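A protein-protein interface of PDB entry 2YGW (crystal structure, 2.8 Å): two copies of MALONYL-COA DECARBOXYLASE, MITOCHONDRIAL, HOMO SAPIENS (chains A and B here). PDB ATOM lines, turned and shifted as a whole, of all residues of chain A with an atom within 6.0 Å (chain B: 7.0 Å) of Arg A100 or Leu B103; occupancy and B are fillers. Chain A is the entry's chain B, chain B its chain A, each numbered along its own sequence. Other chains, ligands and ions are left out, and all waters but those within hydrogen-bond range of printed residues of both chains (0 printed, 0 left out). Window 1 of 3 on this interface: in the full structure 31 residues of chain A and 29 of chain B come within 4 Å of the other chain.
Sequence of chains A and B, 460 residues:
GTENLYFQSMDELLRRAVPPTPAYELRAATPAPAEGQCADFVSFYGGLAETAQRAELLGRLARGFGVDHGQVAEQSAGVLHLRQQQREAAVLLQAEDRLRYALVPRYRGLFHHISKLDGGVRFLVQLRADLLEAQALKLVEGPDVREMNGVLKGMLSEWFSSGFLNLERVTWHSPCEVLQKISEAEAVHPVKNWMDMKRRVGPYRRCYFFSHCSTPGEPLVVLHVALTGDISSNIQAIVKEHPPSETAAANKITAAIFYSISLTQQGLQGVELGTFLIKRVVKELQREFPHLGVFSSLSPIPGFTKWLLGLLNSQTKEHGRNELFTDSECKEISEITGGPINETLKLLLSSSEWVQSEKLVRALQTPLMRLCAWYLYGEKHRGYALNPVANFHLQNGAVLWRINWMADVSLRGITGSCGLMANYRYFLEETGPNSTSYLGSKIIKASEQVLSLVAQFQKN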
ATOM      1  N   LEU A  93      16.679 -28.483  19.249  1.00  0.00           N
ATOM      2  CA  LEU A  93      16.890 -27.096  19.698  1.00  0.00           C
ATOM      3  C   LEU A  93      16.937 -26.085  18.544  1.00  0.00           C
ATOM      4  O   LEU A  93      16.444 -24.966  18.704  1.00  0.00           O
ATOM      5  CB  LEU A  93      18.160 -26.955  20.554  1.00  0.00           C
ATOM      6  CG  LEU A  93      18.206 -27.664  21.919  1.00  0.00           C
ATOM      7  CD1 LEU A  93      19.301 -27.105  22.774  1.00  0.00           C
ATOM      8  CD2 LEU A  93      16.911 -27.551  22.679  1.00  0.00           C
ATOM      9  N   ALA A  95      15.403 -26.462  15.606  1.00  0.00           N
ATOM     10  CA  ALA A  95      14.039 -26.467  15.067  1.00  0.00           C
ATOM     11  C   ALA A  95      13.112 -25.646  15.957  1.00  0.00           C
ATOM     12  O   ALA A  95      12.249 -24.926  15.442  1.00  0.00           O
ATOM     13  CB  ALA A  95      13.533 -27.898  14.929  1.00  0.00           C
ATOM     14  N   GLU A  96      13.330 -25.724  17.288  1.00  0.00           N
ATOM     15  CA  GLU A  96      12.610 -24.965  18.316  1.00  0.00           C
ATOM     16  C   GLU A  96      12.894 -23.475  18.176  1.00  0.00           C
ATOM     17  O   GLU A  96      11.983 -22.671  18.282  1.00  0.00           O
ATOM     18  CB  GLU A  96      13.028 -25.429  19.719  1.00  0.00           C
ATOM     19  CG  GLU A  96      12.425 -26.739  20.182  1.00  0.00           C
ATOM     20  CD  GLU A  96      12.470 -26.942  21.687  1.00  0.00           C
ATOM     21  OE1 GLU A  96      13.298 -26.289  22.362  1.00  0.00           O
ATOM     22  OE2 GLU A  96      11.657 -27.745  22.197  1.00  0.00           O
ATOM     23  N   ASP A  97      14.171 -23.119  17.955  1.00  0.00           N
ATOM     24  CA  ASP A  97      14.655 -21.752  17.758  1.00  0.00           C
ATOM     25  C   ASP A  97      14.096 -21.176  16.451  1.00  0.00           C
ATOM     26  O   ASP A  97      13.736 -19.998  16.426  1.00  0.00           O
ATOM     27  CB  ASP A  97      16.189 -21.725  17.754  1.00  0.00           C
ATOM     28  CG  ASP A  97      16.821 -20.379  18.059  1.00  0.00           C
ATOM     29  OD1 ASP A  97      16.371 -19.711  19.006  1.00  0.00           O
ATOM     30  OD2 ASP A  97      17.831 -20.045  17.426  1.00  0.00           O
ATOM     31  N   ARG A  98      13.998 -21.990  15.376  1.00  0.00           N
ATOM     32  CA  ARG A  98      13.416 -21.512  14.119  1.00  0.00           C
ATOM     33  C   ARG A  98      11.938 -21.113  14.344  1.00  0.00           C
ATOM     34  O   ARG A  98      11.556 -20.008  13.949  1.00  0.00           O
ATOM     35  CB  ARG A  98      13.568 -22.541  13.005  1.00  0.00           C
ATOM     36  CG  ARG A  98      14.969 -22.544  12.429  1.00  0.00           C
ATOM     37  CD  ARG A  98      15.078 -23.481  11.250  1.00  0.00           C
ATOM     38  NE  ARG A  98      15.570 -22.796  10.052  1.00  0.00           N
ATOM     39  CZ  ARG A  98      16.851 -22.707   9.699  1.00  0.00           C
ATOM     40  NH1 ARG A  98      17.798 -23.253  10.459  1.00  0.00           N
ATOM     41  NH2 ARG A  98      17.196 -22.073   8.587  1.00  0.00           N
ATOM     42  N   LEU A  99      11.154 -21.962  15.076  1.00  0.00           N
ATOM     43  CA  LEU A  99       9.770 -21.675  15.499  1.00  0.00           C
ATOM     44  C   LEU A  99       9.719 -20.415  16.396  1.00  0.00           C
ATOM     45  O   LEU A  99       8.803 -19.602  16.247  1.00  0.00           O
ATOM     46  CB  LEU A  99       9.181 -22.894  16.242  1.00  0.00           C
ATOM     47  CG  LEU A  99       7.841 -22.727  16.958  1.00  0.00           C
ATOM     48  CD1 LEU A  99       6.711 -22.416  15.978  1.00  0.00           C
ATOM     49  CD2 LEU A  99       7.529 -23.952  17.762  1.00  0.00           C
ATOM     50  N   ARG A 100      10.706 -20.255  17.309  1.00  0.00           N
ATOM     51  CA  ARG A 100      10.836 -19.113  18.220  1.00  0.00           C
ATOM     52  C   ARG A 100      11.063 -17.842  17.402  1.00  0.00           C
ATOM     53  O   ARG A 100      10.465 -16.801  17.687  1.00  0.00           O
ATOM     54  CB  ARG A 100      11.980 -19.381  19.210  1.00  0.00           C
ATOM     55  CG  ARG A 100      12.335 -18.286  20.214  1.00  0.00           C
ATOM     56  CD  ARG A 100      13.068 -18.784  21.474  1.00  0.00           C
ATOM     57  NE  ARG A 100      14.072 -19.812  21.184  1.00  0.00           N
ATOM     58  CZ  ARG A 100      14.085 -21.040  21.702  1.00  0.00           C
ATOM     59  NH1 ARG A 100      13.171 -21.404  22.594  1.00  0.00           N
ATOM     60  NH2 ARG A 100      15.029 -21.907  21.351  1.00  0.00           N
ATOM     61  N   TYR A 101      11.881 -17.944  16.350  1.00  0.00           N
ATOM     62  CA  TYR A 101      12.193 -16.846  15.433  1.00  0.00           C
ATOM     63  C   TYR A 101      10.968 -16.511  14.551  1.00  0.00           C
ATOM     64  O   TYR A 101      10.712 -15.349  14.276  1.00  0.00           O
ATOM     65  CB  TYR A 101      13.421 -17.204  14.560  1.00  0.00           C
ATOM     66  CG  TYR A 101      13.908 -16.061  13.692  1.00  0.00           C
ATOM     67  CD1 TYR A 101      14.413 -14.889  14.258  1.00  0.00           C
ATOM     68  CD2 TYR A 101      13.826 -16.132  12.302  1.00  0.00           C
ATOM     69  CE1 TYR A 101      14.805 -13.815  13.466  1.00  0.00           C
ATOM     70  CE2 TYR A 101      14.244 -15.067  11.496  1.00  0.00           C
ATOM     71  CZ  TYR A 101      14.745 -13.921  12.087  1.00  0.00           C
ATOM     72  OH  TYR A 101      15.125 -12.860  11.326  1.00  0.00           O
ATOM     73  N   ALA A 102      10.215 -17.532  14.128  1.00  0.00           N
ATOM     74  CA  ALA A 102       9.023 -17.412  13.284  1.00  0.00           C
ATOM     75  C   ALA A 102       7.887 -16.690  14.016  1.00  0.00           C
ATOM     76  O   ALA A 102       7.037 -16.085  13.362  1.00  0.00           O
ATOM     77  CB  ALA A 102       8.569 -18.801  12.835  1.00  0.00           C
ATOM     78  N   LEU A 103       7.897 -16.739  15.371  1.00  0.00           N
ATOM     79  CA  LEU A 103       6.902 -16.133  16.257  1.00  0.00           C
ATOM     80  C   LEU A 103       7.226 -14.670  16.618  1.00  0.00           C
ATOM     81  O   LEU A 103       6.436 -14.024  17.306  1.00  0.00           O
ATOM     82  CB  LEU A 103       6.780 -16.972  17.536  1.00  0.00           C
ATOM     83  CG  LEU A 103       5.967 -18.265  17.455  1.00  0.00           C
ATOM     84  CD1 LEU A 103       6.318 -19.149  18.581  1.00  0.00           C
ATOM     85  CD2 LEU A 103       4.474 -17.991  17.438  1.00  0.00           C
ATOM     86  N   VAL A 104       8.356 -14.130  16.128  1.00  0.00           N
ATOM     87  CA  VAL A 104       8.737 -12.726  16.359  1.00  0.00           C
ATOM     88  C   VAL A 104       8.164 -11.848  15.171  1.00  0.00           C
ATOM     89  O   VAL A 104       8.399 -12.160  13.990  1.00  0.00           O
ATOM     90  CB  VAL A 104      10.261 -12.559  16.618  1.00  0.00           C
ATOM     91  CG1 VAL A 104      11.083 -12.713  15.346  1.00  0.00           C
ATOM     92  CG2 VAL A 104      10.563 -11.236  17.306  1.00  0.00           C
ATOM     93  N   GLY B  66      16.268 -24.464  30.932  1.00  0.00           N
ATOM     94  CA  GLY B  66      15.905 -24.049  29.583  1.00  0.00           C
ATOM     95  C   GLY B  66      14.405 -24.066  29.366  1.00  0.00           C
ATOM     96  O   GLY B  66      13.639 -23.613  30.221  1.00  0.00           O
ATOM     97  N   VAL B  67      13.985 -24.638  28.234  1.00  0.00           N
ATOM     98  CA  VAL B  67      12.598 -24.755  27.783  1.00  0.00           C
ATOM     99  C   VAL B  67      12.001 -26.109  28.219  1.00  0.00           C
ATOM    100  O   VAL B  67      12.720 -27.110  28.289  1.00  0.00           O
ATOM    101  CB  VAL B  67      12.615 -24.576  26.233  1.00  0.00           C
ATOM    102  CG1 VAL B  67      11.579 -25.408  25.511  1.00  0.00           C
ATOM    103  CG2 VAL B  67      12.465 -23.133  25.849  1.00  0.00           C
ATOM    104  N   ASP B  68      10.686 -26.138  28.505  1.00  0.00           N
ATOM    105  CA  ASP B  68       9.966 -27.371  28.805  1.00  0.00           C
ATOM    106  C   ASP B  68       9.564 -27.932  27.438  1.00  0.00           C
ATOM    107  O   ASP B  68       8.562 -27.502  26.853  1.00  0.00           O
ATOM    108  CB  ASP B  68       8.765 -27.088  29.741  1.00  0.00           C
ATOM    109  CG  ASP B  68       7.809 -28.234  30.060  1.00  0.00           C
ATOM    110  OD1 ASP B  68       7.990 -29.347  29.504  1.00  0.00           O
ATOM    111  OD2 ASP B  68       6.867 -28.014  30.854  1.00  0.00           O
ATOM    112  N   VAL B  72       6.024 -27.403  24.795  1.00  0.00           N
ATOM    113  CA  VAL B  72       6.230 -26.815  23.456  1.00  0.00           C
ATOM    114  C   VAL B  72       5.489 -27.645  22.405  1.00  0.00           C
ATOM    115  O   VAL B  72       4.783 -27.075  21.574  1.00  0.00           O
ATOM    116  CB  VAL B  72       7.733 -26.650  23.094  1.00  0.00           C
ATOM    117  CG1 VAL B  72       7.921 -26.160  21.657  1.00  0.00           C
ATOM    118  CG2 VAL B  72       8.421 -25.701  24.059  1.00  0.00           C
ATOM    119  N   SER B  76       2.496 -26.607  20.140  1.00  0.00           N
ATOM    120  CA  SER B  76       2.723 -26.736  18.693  1.00  0.00           C
ATOM    121  C   SER B  76       1.547 -27.488  18.044  1.00  0.00           C
ATOM    122  O   SER B  76       1.048 -27.066  16.996  1.00  0.00           O
ATOM    123  CB  SER B  76       4.039 -27.461  18.410  1.00  0.00           C
ATOM    124  OG  SER B  76       5.177 -26.777  18.910  1.00  0.00           O
ATOM    125  N   GLU B  96      -0.872 -19.185  19.675  1.00  0.00           N
ATOM    126  CA  GLU B  96       0.454 -18.820  19.158  1.00  0.00           C
ATOM    127  C   GLU B  96       1.278 -18.212  20.260  1.00  0.00           C
ATOM    128  O   GLU B  96       2.450 -18.537  20.398  1.00  0.00           O
ATOM    129  CB  GLU B  96       0.328 -17.831  17.999  1.00  0.00           C
ATOM    130  CG  GLU B  96      -0.093 -18.463  16.687  1.00  0.00           C
ATOM    131  CD  GLU B  96       0.169 -17.598  15.475  1.00  0.00           C
ATOM    132  OE1 GLU B  96       0.401 -16.373  15.636  1.00  0.00           O
ATOM    133  OE2 GLU B  96       0.128 -18.156  14.355  1.00  0.00           O
ATOM    134  N   ASP B  97       0.658 -17.322  21.054  1.00  0.00           N
ATOM    135  CA  ASP B  97       1.258 -16.658  22.209  1.00  0.00           C
ATOM    136  C   ASP B  97       1.580 -17.692  23.313  1.00  0.00           C
ATOM    137  O   ASP B  97       2.624 -17.577  23.952  1.00  0.00           O
ATOM    138  CB  ASP B  97       0.307 -15.572  22.723  1.00  0.00           C
ATOM    139  CG  ASP B  97       0.934 -14.499  23.571  1.00  0.00           C
ATOM    140  OD1 ASP B  97       2.051 -14.040  23.231  1.00  0.00           O
ATOM    141  OD2 ASP B  97       0.277 -14.048  24.518  1.00  0.00           O
ATOM    142  N   ARG B  98       0.714 -18.750  23.472  1.00  0.00           N
ATOM    143  CA  ARG B  98       0.886 -19.864  24.434  1.00  0.00           C
ATOM    144  C   ARG B  98       2.160 -20.635  24.140  1.00  0.00           C
ATOM    145  O   ARG B  98       2.895 -21.008  25.059  1.00  0.00           O
ATOM    146  CB  ARG B  98      -0.304 -20.821  24.412  1.00  0.00           C
ATOM    147  CG  ARG B  98      -1.426 -20.378  25.307  1.00  0.00           C
ATOM    148  CD  ARG B  98      -2.072 -21.527  26.034  1.00  0.00           C
ATOM    149  NE  ARG B  98      -3.155 -21.040  26.882  1.00  0.00           N
ATOM    150  CZ  ARG B  98      -4.396 -20.828  26.458  1.00  0.00           C
ATOM    151  NH1 ARG B  98      -4.724 -21.067  25.194  1.00  0.00           N
ATOM    152  NH2 ARG B  98      -5.319 -20.378  27.294  1.00  0.00           N
ATOM    153  N   LEU B  99       2.415 -20.859  22.844  1.00  0.00           N
ATOM    154  CA  LEU B  99       3.609 -21.493  22.293  1.00  0.00           C
ATOM    155  C   LEU B  99       4.810 -20.566  22.401  1.00  0.00           C
ATOM    156  O   LEU B  99       5.902 -21.047  22.706  1.00  0.00           O
ATOM    157  CB  LEU B  99       3.349 -21.866  20.830  1.00  0.00           C
ATOM    158  CG  LEU B  99       4.516 -22.368  19.982  1.00  0.00           C
ATOM    159  CD1 LEU B  99       5.096 -23.679  20.537  1.00  0.00           C
ATOM    160  CD2 LEU B  99       4.066 -22.549  18.561  1.00  0.00           C
ATOM    161  N   ARG B 100       4.618 -19.249  22.160  1.00  0.00           N
ATOM    162  CA  ARG B 100       5.658 -18.213  22.252  1.00  0.00           C
ATOM    163  C   ARG B 100       6.161 -18.147  23.684  1.00  0.00           C
ATOM    164  O   ARG B 100       7.367 -18.081  23.886  1.00  0.00           O
ATOM    165  CB  ARG B 100       5.089 -16.860  21.775  1.00  0.00           C
ATOM    166  CG  ARG B 100       5.964 -15.617  21.896  1.00  0.00           C
ATOM    167  CD  ARG B 100       5.572 -14.460  20.932  1.00  0.00           C
ATOM    168  NE  ARG B 100       4.115 -14.277  20.824  1.00  0.00           N
ATOM    169  CZ  ARG B 100       3.421 -14.351  19.689  1.00  0.00           C
ATOM    170  NH1 ARG B 100       4.044 -14.541  18.533  1.00  0.00           N
ATOM    171  NH2 ARG B 100       2.098 -14.208  19.700  1.00  0.00           N
ATOM    172  N   TYR B 101       5.248 -18.244  24.665  1.00  0.00           N
ATOM    173  CA  TYR B 101       5.545 -18.209  26.098  1.00  0.00           C
ATOM    174  C   TYR B 101       6.279 -19.486  26.525  1.00  0.00           C
ATOM    175  O   TYR B 101       7.212 -19.431  27.328  1.00  0.00           O
ATOM    176  CB  TYR B 101       4.225 -18.021  26.903  1.00  0.00           C
ATOM    177  CG  TYR B 101       4.424 -17.747  28.377  1.00  0.00           C
ATOM    178  CD1 TYR B 101       4.853 -16.506  28.821  1.00  0.00           C
ATOM    179  CD2 TYR B 101       4.160 -18.722  29.331  1.00  0.00           C
ATOM    180  CE1 TYR B 101       5.047 -16.245  30.178  1.00  0.00           C
ATOM    181  CE2 TYR B 101       4.371 -18.481  30.689  1.00  0.00           C
ATOM    182  CZ  TYR B 101       4.814 -17.237  31.111  1.00  0.00           C
ATOM    183  OH  TYR B 101       5.024 -16.974  32.450  1.00  0.00           O
ATOM    184  N   ALA B 102       5.859 -20.638  25.965  1.00  0.00           N
ATOM    185  CA  ALA B 102       6.419 -21.970  26.250  1.00  0.00           C
ATOM    186  C   ALA B 102       7.863 -22.125  25.763  1.00  0.00           C
ATOM    187  O   ALA B 102       8.633 -22.923  26.335  1.00  0.00           O
ATOM    188  CB  ALA B 102       5.564 -23.017  25.602  1.00  0.00           C
ATOM    189  N   LEU B 103       8.229 -21.335  24.723  1.00  0.00           N
ATOM    190  CA  LEU B 103       9.545 -21.329  24.088  1.00  0.00           C
ATOM    191  C   LEU B 103      10.528 -20.404  24.777  1.00  0.00           C
ATOM    192  O   LEU B 103      11.677 -20.331  24.339  1.00  0.00           O
ATOM    193  CB  LEU B 103       9.416 -20.914  22.617  1.00  0.00           C
ATOM    194  CG  LEU B 103       8.956 -21.962  21.635  1.00  0.00           C
ATOM    195  CD1 LEU B 103       8.469 -21.299  20.397  1.00  0.00           C
ATOM    196  CD2 LEU B 103      10.073 -22.952  21.308  1.00  0.00           C
ATOM    197  N   VAL B 104      10.096 -19.684  25.837  1.00  0.00           N
ATOM    198  CA  VAL B 104      10.980 -18.770  26.563  1.00  0.00           C
ATOM    199  C   VAL B 104      11.672 -19.587  27.712  1.00  0.00           C
ATOM    200  O   VAL B 104      10.970 -20.211  28.523  1.00  0.00           O
ATOM    201  CB  VAL B 104      10.256 -17.465  27.009  1.00  0.00           C
ATOM    202  CG1 VAL B 104       9.288 -17.675  28.166  1.00  0.00           C
ATOM    203  CG2 VAL B 104      11.245 -16.389  27.346  1.00  0.00           C
ATOM    204  N   PRO B 105      13.039 -19.701  27.695  1.00  0.00           N
ATOM    205  CA  PRO B 105      13.731 -20.514  28.710  1.00  0.00           C
ATOM    206  C   PRO B 105      13.680 -19.880  30.084  1.00  0.00           C
ATOM    207  O   PRO B 105      13.669 -18.659  30.184  1.00  0.00           O
ATOM    208  CB  PRO B 105      15.156 -20.589  28.187  1.00  0.00           C
ATOM    209  CG  PRO B 105      15.314 -19.395  27.377  1.00  0.00           C
ATOM    210  CD  PRO B 105      14.005 -19.109  26.752  1.00  0.00           C
ATOM    211  N   TYR B 107      15.971 -19.552  32.350  1.00  0.00           N
ATOM    212  CA  TYR B 107      17.143 -18.723  32.685  1.00  0.00           C
ATOM    213  C   TYR B 107      16.992 -17.300  32.216  1.00  0.00           C
ATOM    214  O   TYR B 107      17.562 -16.420  32.848  1.00  0.00           O
ATOM    215  CB  TYR B 107      18.494 -19.282  32.188  1.00  0.00           C
ATOM    216  CG  TYR B 107      18.548 -19.832  30.779  1.00  0.00           C
ATOM    217  CD1 TYR B 107      18.602 -18.985  29.679  1.00  0.00           C
ATOM    218  CD2 TYR B 107      18.691 -21.192  30.550  1.00  0.00           C
ATOM    219  CE1 TYR B 107      18.696 -19.489  28.382  1.00  0.00           C
ATOM    220  CE2 TYR B 107      18.773 -21.709  29.261  1.00  0.00           C
ATOM    221  CZ  TYR B 107      18.780 -20.855  28.179  1.00  0.00           C
ATOM    222  OH  TYR B 107      18.846 -21.394  26.917  1.00  0.00           O
ATOM    223  N   GLU B 147      22.673 -22.299  23.123  1.00  0.00           N
ATOM    224  CA  GLU B 147      21.356 -21.641  23.171  1.00  0.00           C
ATOM    225  C   GLU B 147      21.376 -20.507  24.170  1.00  0.00           C
ATOM    226  O   GLU B 147      20.954 -19.407  23.822  1.00  0.00           O
ATOM    227  CB  GLU B 147      20.248 -22.641  23.539  1.00  0.00           C
ATOM    228  CG  GLU B 147      19.801 -23.516  22.385  1.00  0.00           C
ATOM    229  CD  GLU B 147      18.844 -22.873  21.407  1.00  0.00           C
ATOM    230  OE1 GLU B 147      17.659 -22.717  21.777  1.00  0.00           O
ATOM    231  OE2 GLU B 147      19.285 -22.491  20.297  1.00  0.00           O
ATOM    232  N   VAL B 151      20.771 -16.380  23.758  1.00  0.00           N
ATOM    233  CA  VAL B 151      19.747 -15.708  24.588  1.00  0.00           C
ATOM    234  C   VAL B 151      20.373 -14.474  25.228  1.00  0.00           C
ATOM    235  O   VAL B 151      19.755 -13.419  25.234  1.00  0.00           O
ATOM    236  CB  VAL B 151      19.129 -16.677  25.655  1.00  0.00           C
ATOM    237  CG1 VAL B 151      18.434 -15.933  26.796  1.00  0.00           C
ATOM    238  CG2 VAL B 151      18.190 -17.691  25.016  1.00  0.00           C
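Among the printed residues, merely in contact across the chains: Leu A103 with Leu B103, Glu A96 with Leu B103, Leu A103 with Glu B96, Leu A93 with Glu B147, Glu A96 with Val B67, Leu A99 with Leu B99, Arg A100 with Val B67, Leu A99 with Leu B103, Leu A99 with Ser B76, Asp A97 with Glu B147 and Leu A103 with Leu B99.
The backbone carbonyl oxygen (O) of Leu A103 lies within hydrogen-bond range of the guanidinium group (NH1) of Arg B100, at 2.7 Å.
O of Leu B103 is in hydrogen-bond range of NH1 of Arg A100.
OE1 of Glu B147 lies within salt-bridge range of NH2 of Arg A100, at 2.8 Å.
Glu A96 touches Leu B103, and with the chains exchanged Leu A103 touches Glu B96.
Leu B99 touches its own counterpart, Leu A99.
Arg A100 touches Leu B103, and with the chains exchanged Leu A103 touches Arg B100.
Leu B103 touches its own counterpart, Leu A103.
Positions printed for both chains: 96, 97, 98, 99, 100, 101, 102, 103 and 104.
Of the 14 pairs that touch across the chains among the printed residues, 8 have their exchanged pair printed and touching as well.
Hydrophobic or aromatic side chains of chain A within 4 Å of the printed part of chain B: Leu A93, Leu A99 and Leu A103.
Of the 18 printed residues of chain B, 7 touch a printed residue of chain A.
Hydrophobic or aromatic side chains of chain B within 4 Å of the printed part of chain A: Val B67, Leu B99 and Leu B103.
Among the printed residues, Asp or Glu carboxylates within 4 Å of a Lys or Arg side-chain nitrogen of the other chain: Arg A100 with Glu B147 (2.8 Å).
Printed residues of chain B within 4 Å of Leu A93: Glu B147.
Printed residues of chain B within 4 Å of Glu A96: Val B67 (3.7 Å) and Leu B103 (3.6 Å).
Of the printed residues of chain B, Asp A97 touches Glu B147.
Printed residues of chain B within 4 Å of Leu A99: Ser B76, Leu B99 and Leu B103.
Arg A100 touches just these residues of chain B: Val B67, Leu B103 and Glu B147.
Ala A102 touches none of the printed residues of chain B.
Of the printed residues of chain A, Val B67 touches Glu A96 and Arg A100.
Ala B102 touches none of the printed residues of chain A.
Leu B103 touches four residues of chain A.
The nearest residue of chain B that does not touch Arg A100 is Val B104 (4.8 Å).
O of Val B72 sits at hydrogen-bond distance from OG of Ser B76 (2.7 Å).
OD1 of Asp B97 lies within salt-bridge range of NE of Arg B100, at 3.2 Å.
The side-chain carboxylate (OD1) of Asp A97 is in salt-bridge range of the guanidinium group (NE) of Arg A100 (3.2 Å).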
